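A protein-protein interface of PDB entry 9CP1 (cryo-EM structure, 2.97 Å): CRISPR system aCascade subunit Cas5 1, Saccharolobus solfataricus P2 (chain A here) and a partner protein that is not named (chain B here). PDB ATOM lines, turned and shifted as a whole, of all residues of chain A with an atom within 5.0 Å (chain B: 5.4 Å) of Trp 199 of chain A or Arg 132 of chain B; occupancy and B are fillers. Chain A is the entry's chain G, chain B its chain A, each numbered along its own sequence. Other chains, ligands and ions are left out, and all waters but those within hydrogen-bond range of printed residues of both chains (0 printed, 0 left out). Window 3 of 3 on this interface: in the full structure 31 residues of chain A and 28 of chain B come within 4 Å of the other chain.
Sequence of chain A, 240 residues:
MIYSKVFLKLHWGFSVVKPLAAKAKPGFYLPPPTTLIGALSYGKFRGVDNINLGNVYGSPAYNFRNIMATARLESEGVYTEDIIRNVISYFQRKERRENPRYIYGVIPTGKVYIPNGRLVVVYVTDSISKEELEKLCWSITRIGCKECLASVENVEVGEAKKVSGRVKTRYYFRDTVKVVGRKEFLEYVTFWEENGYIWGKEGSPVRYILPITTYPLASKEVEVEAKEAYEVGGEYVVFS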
ATOM      1  N   ASP A  49      -5.339  34.975 -10.461  1.00  0.00           N
ATOM      2  CA  ASP A  49      -5.117  33.550 -10.652  1.00  0.00           C
ATOM      3  C   ASP A  49      -6.341  32.788 -11.129  1.00  0.00           C
ATOM      4  O   ASP A  49      -6.191  31.651 -11.588  1.00  0.00           O
ATOM      5  CB  ASP A  49      -4.619  32.902  -9.351  1.00  0.00           C
ATOM      6  CG  ASP A  49      -3.374  33.564  -8.808  1.00  0.00           C
ATOM      7  OD1 ASP A  49      -2.718  34.308  -9.564  1.00  0.00           O
ATOM      8  OD2 ASP A  49      -3.051  33.345  -7.622  1.00  0.00           O
ATOM      9  N   ASN A  50      -7.535  33.367 -11.034  1.00  0.00           N
ATOM     10  CA  ASN A  50      -8.753  32.707 -11.492  1.00  0.00           C
ATOM     11  C   ASN A  50      -9.670  33.744 -12.116  1.00  0.00           C
ATOM     12  O   ASN A  50     -10.062  34.708 -11.453  1.00  0.00           O
ATOM     13  CB  ASN A  50      -9.462  31.990 -10.339  1.00  0.00           C
ATOM     14  CG  ASN A  50      -8.728  30.746  -9.889  1.00  0.00           C
ATOM     15  OD1 ASN A  50      -8.263  29.955 -10.709  1.00  0.00           O
ATOM     16  ND2 ASN A  50      -8.624  30.562  -8.579  1.00  0.00           N
ATOM     17  N   TYR A  57     -13.924  28.224 -13.952  1.00  0.00           N
ATOM     18  CA  TYR A  57     -12.658  28.884 -13.655  1.00  0.00           C
ATOM     19  C   TYR A  57     -11.522  27.971 -14.098  1.00  0.00           C
ATOM     20  O   TYR A  57     -11.261  26.950 -13.455  1.00  0.00           O
ATOM     21  CB  TYR A  57     -12.550  29.171 -12.160  1.00  0.00           C
ATOM     22  CG  TYR A  57     -13.295  30.394 -11.679  1.00  0.00           C
ATOM     23  CD1 TYR A  57     -12.782  31.667 -11.879  1.00  0.00           C
ATOM     24  CD2 TYR A  57     -14.505  30.272 -11.010  1.00  0.00           C
ATOM     25  CE1 TYR A  57     -13.456  32.787 -11.432  1.00  0.00           C
ATOM     26  CE2 TYR A  57     -15.187  31.386 -10.561  1.00  0.00           C
ATOM     27  CZ  TYR A  57     -14.658  32.641 -10.775  1.00  0.00           C
ATOM     28  OH  TYR A  57     -15.331  33.756 -10.332  1.00  0.00           O
ATOM     29  N   GLY A  58     -10.845  28.313 -15.193  1.00  0.00           N
ATOM     30  CA  GLY A  58      -9.754  27.452 -15.605  1.00  0.00           C
ATOM     31  C   GLY A  58      -8.364  28.056 -15.616  1.00  0.00           C
ATOM     32  O   GLY A  58      -7.410  27.378 -15.228  1.00  0.00           O
ATOM     33  N   SER A  59      -8.231  29.323 -16.020  1.00  0.00           N
ATOM     34  CA  SER A  59      -6.946  30.020 -16.011  1.00  0.00           C
ATOM     35  C   SER A  59      -7.113  31.453 -16.495  1.00  0.00           C
ATOM     36  O   SER A  59      -8.027  31.736 -17.281  1.00  0.00           O
ATOM     37  CB  SER A  59      -5.920  29.306 -16.893  1.00  0.00           C
ATOM     38  OG  SER A  59      -6.420  29.121 -18.204  1.00  0.00           O
ATOM     39  N   PRO A  60      -6.253  32.381 -16.071  1.00  0.00           N
ATOM     40  CA  PRO A  60      -6.179  33.705 -16.704  1.00  0.00           C
ATOM     41  C   PRO A  60      -5.282  33.712 -17.939  1.00  0.00           C
ATOM     42  O   PRO A  60      -4.455  34.604 -18.126  1.00  0.00           O
ATOM     43  CB  PRO A  60      -5.607  34.586 -15.588  1.00  0.00           C
ATOM     44  CG  PRO A  60      -5.600  33.735 -14.344  1.00  0.00           C
ATOM     45  CD  PRO A  60      -5.468  32.338 -14.833  1.00  0.00           C
ATOM     46  N   TYR A 197      -5.887  24.186 -20.454  1.00  0.00           N
ATOM     47  CA  TYR A 197      -5.815  25.363 -19.596  1.00  0.00           C
ATOM     48  C   TYR A 197      -6.824  25.321 -18.456  1.00  0.00           C
ATOM     49  O   TYR A 197      -6.668  26.064 -17.482  1.00  0.00           O
ATOM     50  CB  TYR A 197      -6.024  26.631 -20.425  1.00  0.00           C
ATOM     51  CG  TYR A 197      -4.745  27.234 -20.957  1.00  0.00           C
ATOM     52  CD1 TYR A 197      -3.777  27.725 -20.094  1.00  0.00           C
ATOM     53  CD2 TYR A 197      -4.509  27.321 -22.320  1.00  0.00           C
ATOM     54  CE1 TYR A 197      -2.608  28.281 -20.573  1.00  0.00           C
ATOM     55  CE2 TYR A 197      -3.343  27.876 -22.810  1.00  0.00           C
ATOM     56  CZ  TYR A 197      -2.398  28.356 -21.931  1.00  0.00           C
ATOM     57  OH  TYR A 197      -1.233  28.909 -22.410  1.00  0.00           O
ATOM     58  N   ILE A 198      -7.847  24.478 -18.548  1.00  0.00           N
ATOM     59  CA  ILE A 198      -8.890  24.390 -17.530  1.00  0.00           C
ATOM     60  C   ILE A 198      -8.561  23.255 -16.571  1.00  0.00           C
ATOM     61  O   ILE A 198      -8.194  22.154 -16.997  1.00  0.00           O
ATOM     62  CB  ILE A 198     -10.272  24.186 -18.180  1.00  0.00           C
ATOM     63  CG1 ILE A 198     -10.663  25.408 -19.011  1.00  0.00           C
ATOM     64  CG2 ILE A 198     -11.326  23.899 -17.123  1.00  0.00           C
ATOM     65  CD1 ILE A 198     -10.357  25.274 -20.485  1.00  0.00           C
ATOM     66  N   TRP A 199      -8.697  23.517 -15.271  1.00  0.00           N
ATOM     67  CA  TRP A 199      -8.394  22.501 -14.274  1.00  0.00           C
ATOM     68  C   TRP A 199      -9.344  21.312 -14.398  1.00  0.00           C
ATOM     69  O   TRP A 199     -10.438  21.408 -14.959  1.00  0.00           O
ATOM     70  CB  TRP A 199      -8.484  23.064 -12.856  1.00  0.00           C
ATOM     71  CG  TRP A 199      -8.044  24.478 -12.699  1.00  0.00           C
ATOM     72  CD1 TRP A 199      -8.823  25.543 -12.367  1.00  0.00           C
ATOM     73  CD2 TRP A 199      -6.713  24.984 -12.844  1.00  0.00           C
ATOM     74  NE1 TRP A 199      -8.064  26.685 -12.304  1.00  0.00           N
ATOM     75  CE2 TRP A 199      -6.762  26.367 -12.589  1.00  0.00           C
ATOM     76  CE3 TRP A 199      -5.485  24.402 -13.167  1.00  0.00           C
ATOM     77  CZ2 TRP A 199      -5.634  27.179 -12.654  1.00  0.00           C
ATOM     78  CZ3 TRP A 199      -4.366  25.209 -13.228  1.00  0.00           C
ATOM     79  CH2 TRP A 199      -4.448  26.581 -12.973  1.00  0.00           C
ATOM     80  N   GLY A 200      -8.905  20.180 -13.855  1.00  0.00           N
ATOM     81  CA  GLY A 200      -9.709  18.972 -13.890  1.00  0.00           C
ATOM     82  C   GLY A 200      -9.981  18.459 -15.285  1.00  0.00           C
ATOM     83  O   GLY A 200     -11.032  17.854 -15.524  1.00  0.00           O
ATOM     84  N   LYS A 201      -9.058  18.682 -16.216  1.00  0.00           N
ATOM     85  CA  LYS A 201      -9.241  18.251 -17.593  1.00  0.00           C
ATOM     86  C   LYS A 201      -7.874  18.138 -18.249  1.00  0.00           C
ATOM     87  O   LYS A 201      -6.988  18.956 -17.990  1.00  0.00           O
ATOM     88  CB  LYS A 201     -10.133  19.228 -18.364  1.00  0.00           C
ATOM     89  CG  LYS A 201     -10.652  18.692 -19.684  1.00  0.00           C
ATOM     90  CD  LYS A 201     -10.926  19.825 -20.653  1.00  0.00           C
ATOM     91  CE  LYS A 201     -11.845  20.863 -20.033  1.00  0.00           C
ATOM     92  NZ  LYS A 201     -12.125  21.987 -20.968  1.00  0.00           N
ATOM     93  N   GLU B 108     -11.324  32.425   0.407  1.00  0.00           N
ATOM     94  CA  GLU B 108      -9.983  32.979   0.276  1.00  0.00           C
ATOM     95  C   GLU B 108      -9.764  34.113   1.266  1.00  0.00           C
ATOM     96  O   GLU B 108      -8.719  34.190   1.916  1.00  0.00           O
ATOM     97  CB  GLU B 108      -9.748  33.468  -1.152  1.00  0.00           C
ATOM     98  CG  GLU B 108      -8.382  34.102  -1.356  1.00  0.00           C
ATOM     99  CD  GLU B 108      -8.057  34.337  -2.817  1.00  0.00           C
ATOM    100  OE1 GLU B 108      -8.939  34.106  -3.670  1.00  0.00           O
ATOM    101  OE2 GLU B 108      -6.918  34.757  -3.112  1.00  0.00           O
ATOM    102  N   PHE B 123      -1.003  29.505  -0.667  1.00  0.00           N
ATOM    103  CA  PHE B 123      -1.548  28.213  -0.289  1.00  0.00           C
ATOM    104  C   PHE B 123      -2.287  27.609  -1.470  1.00  0.00           C
ATOM    105  O   PHE B 123      -2.624  28.298  -2.436  1.00  0.00           O
ATOM    106  CB  PHE B 123      -2.492  28.330   0.914  1.00  0.00           C
ATOM    107  CG  PHE B 123      -3.773  29.056   0.613  1.00  0.00           C
ATOM    108  CD1 PHE B 123      -4.887  28.369   0.160  1.00  0.00           C
ATOM    109  CD2 PHE B 123      -3.868  30.422   0.793  1.00  0.00           C
ATOM    110  CE1 PHE B 123      -6.061  29.032  -0.118  1.00  0.00           C
ATOM    111  CE2 PHE B 123      -5.044  31.090   0.517  1.00  0.00           C
ATOM    112  CZ  PHE B 123      -6.140  30.393   0.063  1.00  0.00           C
ATOM    113  N   MET B 124      -2.536  26.306  -1.379  1.00  0.00           N
ATOM    114  CA  MET B 124      -3.396  25.610  -2.323  1.00  0.00           C
ATOM    115  C   MET B 124      -4.283  24.645  -1.558  1.00  0.00           C
ATOM    116  O   MET B 124      -3.797  23.896  -0.705  1.00  0.00           O
ATOM    117  CB  MET B 124      -2.581  24.854  -3.376  1.00  0.00           C
ATOM    118  CG  MET B 124      -3.392  24.442  -4.590  1.00  0.00           C
ATOM    119  SD  MET B 124      -2.932  22.815  -5.209  1.00  0.00           S
ATOM    120  CE  MET B 124      -3.584  21.768  -3.912  1.00  0.00           C
ATOM    121  N   PRO B 130     -11.170  23.883  -5.860  1.00  0.00           N
ATOM    122  CA  PRO B 130      -9.826  24.303  -5.452  1.00  0.00           C
ATOM    123  C   PRO B 130      -9.673  25.815  -5.465  1.00  0.00           C
ATOM    124  O   PRO B 130     -10.284  26.521  -6.271  1.00  0.00           O
ATOM    125  CB  PRO B 130      -8.919  23.646  -6.496  1.00  0.00           C
ATOM    126  CG  PRO B 130      -9.795  23.477  -7.692  1.00  0.00           C
ATOM    127  CD  PRO B 130     -11.162  23.175  -7.151  1.00  0.00           C
ATOM    128  N   VAL B 131      -8.842  26.305  -4.550  1.00  0.00           N
ATOM    129  CA  VAL B 131      -8.503  27.718  -4.454  1.00  0.00           C
ATOM    130  C   VAL B 131      -6.988  27.842  -4.508  1.00  0.00           C
ATOM    131  O   VAL B 131      -6.271  27.033  -3.908  1.00  0.00           O
ATOM    132  CB  VAL B 131      -9.059  28.358  -3.165  1.00  0.00           C
ATOM    133  CG1 VAL B 131      -8.951  29.870  -3.235  1.00  0.00           C
ATOM    134  CG2 VAL B 131     -10.499  27.935  -2.940  1.00  0.00           C
ATOM    135  N   ARG B 132      -6.499  28.851  -5.223  1.00  0.00           N
ATOM    136  CA  ARG B 132      -5.073  29.007  -5.461  1.00  0.00           C
ATOM    137  C   ARG B 132      -4.612  30.382  -5.004  1.00  0.00           C
ATOM    138  O   ARG B 132      -5.383  31.345  -4.976  1.00  0.00           O
ATOM    139  CB  ARG B 132      -4.726  28.831  -6.941  1.00  0.00           C
ATOM    140  CG  ARG B 132      -5.309  27.597  -7.590  1.00  0.00           C
ATOM    141  CD  ARG B 132      -4.575  27.301  -8.879  1.00  0.00           C
ATOM    142  NE  ARG B 132      -4.450  28.492  -9.707  1.00  0.00           N
ATOM    143  CZ  ARG B 132      -3.471  28.699 -10.577  1.00  0.00           C
ATOM    144  NH1 ARG B 132      -2.510  27.810 -10.759  1.00  0.00           N
ATOM    145  NH2 ARG B 132      -3.456  29.826 -11.281  1.00  0.00           N
ATOM    146  N   ARG B 133      -3.331  30.462  -4.651  1.00  0.00           N
ATOM    147  CA  ARG B 133      -2.704  31.742  -4.331  1.00  0.00           C
ATOM    148  C   ARG B 133      -1.202  31.585  -4.522  1.00  0.00           C
ATOM    149  O   ARG B 133      -0.558  30.856  -3.764  1.00  0.00           O
ATOM    150  CB  ARG B 133      -3.036  32.177  -2.911  1.00  0.00           C
ATOM    151  CG  ARG B 133      -2.396  33.497  -2.531  1.00  0.00           C
ATOM    152  CD  ARG B 133      -3.197  34.232  -1.478  1.00  0.00           C
ATOM    153  NE  ARG B 133      -2.606  35.528  -1.166  1.00  0.00           N
ATOM    154  CZ  ARG B 133      -2.841  36.640  -1.847  1.00  0.00           C
ATOM    155  NH1 ARG B 133      -3.676  36.659  -2.871  1.00  0.00           N
ATOM    156  NH2 ARG B 133      -2.221  37.761  -1.492  1.00  0.00           N
ATOM    157  N   THR B 134      -0.654  32.266  -5.524  1.00  0.00           N
ATOM    158  CA  THR B 134       0.773  32.183  -5.795  1.00  0.00           C
ATOM    159  C   THR B 134       1.566  32.954  -4.744  1.00  0.00           C
ATOM    160  O   THR B 134       1.112  33.969  -4.211  1.00  0.00           O
ATOM    161  CB  THR B 134       1.081  32.725  -7.190  1.00  0.00           C
ATOM    162  OG1 THR B 134       0.160  32.162  -8.131  1.00  0.00           O
ATOM    163  CG2 THR B 134       2.495  32.362  -7.610  1.00  0.00           C
ATOM    164  N   SER B 199      -6.919  37.358  -4.679  1.00  0.00           N
ATOM    165  CA  SER B 199      -6.497  36.967  -6.018  1.00  0.00           C
ATOM    166  C   SER B 199      -7.561  36.147  -6.735  1.00  0.00           C
ATOM    167  O   SER B 199      -7.258  35.093  -7.304  1.00  0.00           O
ATOM    168  CB  SER B 199      -5.188  36.183  -5.949  1.00  0.00           C
ATOM    169  OG  SER B 199      -4.781  35.768  -7.238  1.00  0.00           O
ATOM    170  N   THR B 200      -8.806  36.614  -6.712  1.00  0.00           N
ATOM    171  CA  THR B 200      -9.890  35.945  -7.421  1.00  0.00           C
ATOM    172  C   THR B 200     -10.950  36.974  -7.784  1.00  0.00           C
ATOM    173  O   THR B 200     -11.324  37.800  -6.947  1.00  0.00           O
ATOM    174  CB  THR B 200     -10.508  34.826  -6.573  1.00  0.00           C
ATOM    175  OG1 THR B 200      -9.469  34.012  -6.017  1.00  0.00           O
ATOM    176  CG2 THR B 200     -11.418  33.959  -7.424  1.00  0.00           C
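The side-chain hydroxyl of Ser 199 of chain B sits at hydrogen-bond distance from the side-chain carboxylate of Asp 49 of chain A. NH2 of Arg 132 of chain B lies within hydrogen-bond range of O of Asp 49 of chain A (3.3 Å). N of Thr 134 of chain B sits at hydrogen-bond distance from OD2 of Asp 49 of chain A (3.4 Å).
The backbone NH of Ser 199 of chain B sits at hydrogen-bond distance from the side-chain carboxylate of Glu 108 of chain B, at 3.0 Å. The backbone carbonyl oxygen (O) of Tyr 57 of chain A sits close to the indole nitrogen (NE1) of Trp 199 of chain A. OE2 of Glu 108 of chain B lies within salt-bridge range of NH1 of Arg 133 of chain B, 3.8 Å away. O of Gly 58 of chain A lies close to NE1 of Trp 199 of chain A, at 3.1 Å. O of Phe 123 of chain B sits at hydrogen-bond distance from N of Arg 133 of chain B, at 3.2 Å.
Among the printed residues, merely in contact across the chains: Trp 199 of chain A with Arg 132 of chain B and Asp 49 of chain A with Arg 133 of chain B.
Of chain B, only Arg 132 comes within 4 Å of Trp 199 of chain A. Printed residues of chain A within 4 Å of Arg 132 of chain B: Asp 49 and Trp 199. Of the printed residues of chain A, Arg 133 of chain B touches Asp 49. Of the printed residues of chain A, Thr 134 of chain B touches Asp 49 (3.4 Å). Of the printed residues of chain A, Ser 199 of chain B touches Asp 49. Of the printed residues of chain B, Asp 49 of chain A touches Arg 132 (3.3 Å), Arg 133 (3.7 Å), Thr 134 (3.4 Å) and Ser 199 (3.0 Å). The nearest residue of chain B that does not touch Trp 199 of chain A is Pro 130 of chain B (5.2 Å).
Printed residues of chain A that touch a printed residue of chain B: Asp 49 and Trp 199. Printed residues of chain B that touch a printed residue of chain A: Arg 132, Arg 133, Thr 134 and Ser 199. Along chain B the printed residues that touch a printed residue of chain A span positions 132 to 199. Among the printed residues, no Asp or Glu carboxylate lies within 4 Å of a Lys or Arg side-chain nitrogen of the other chain.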
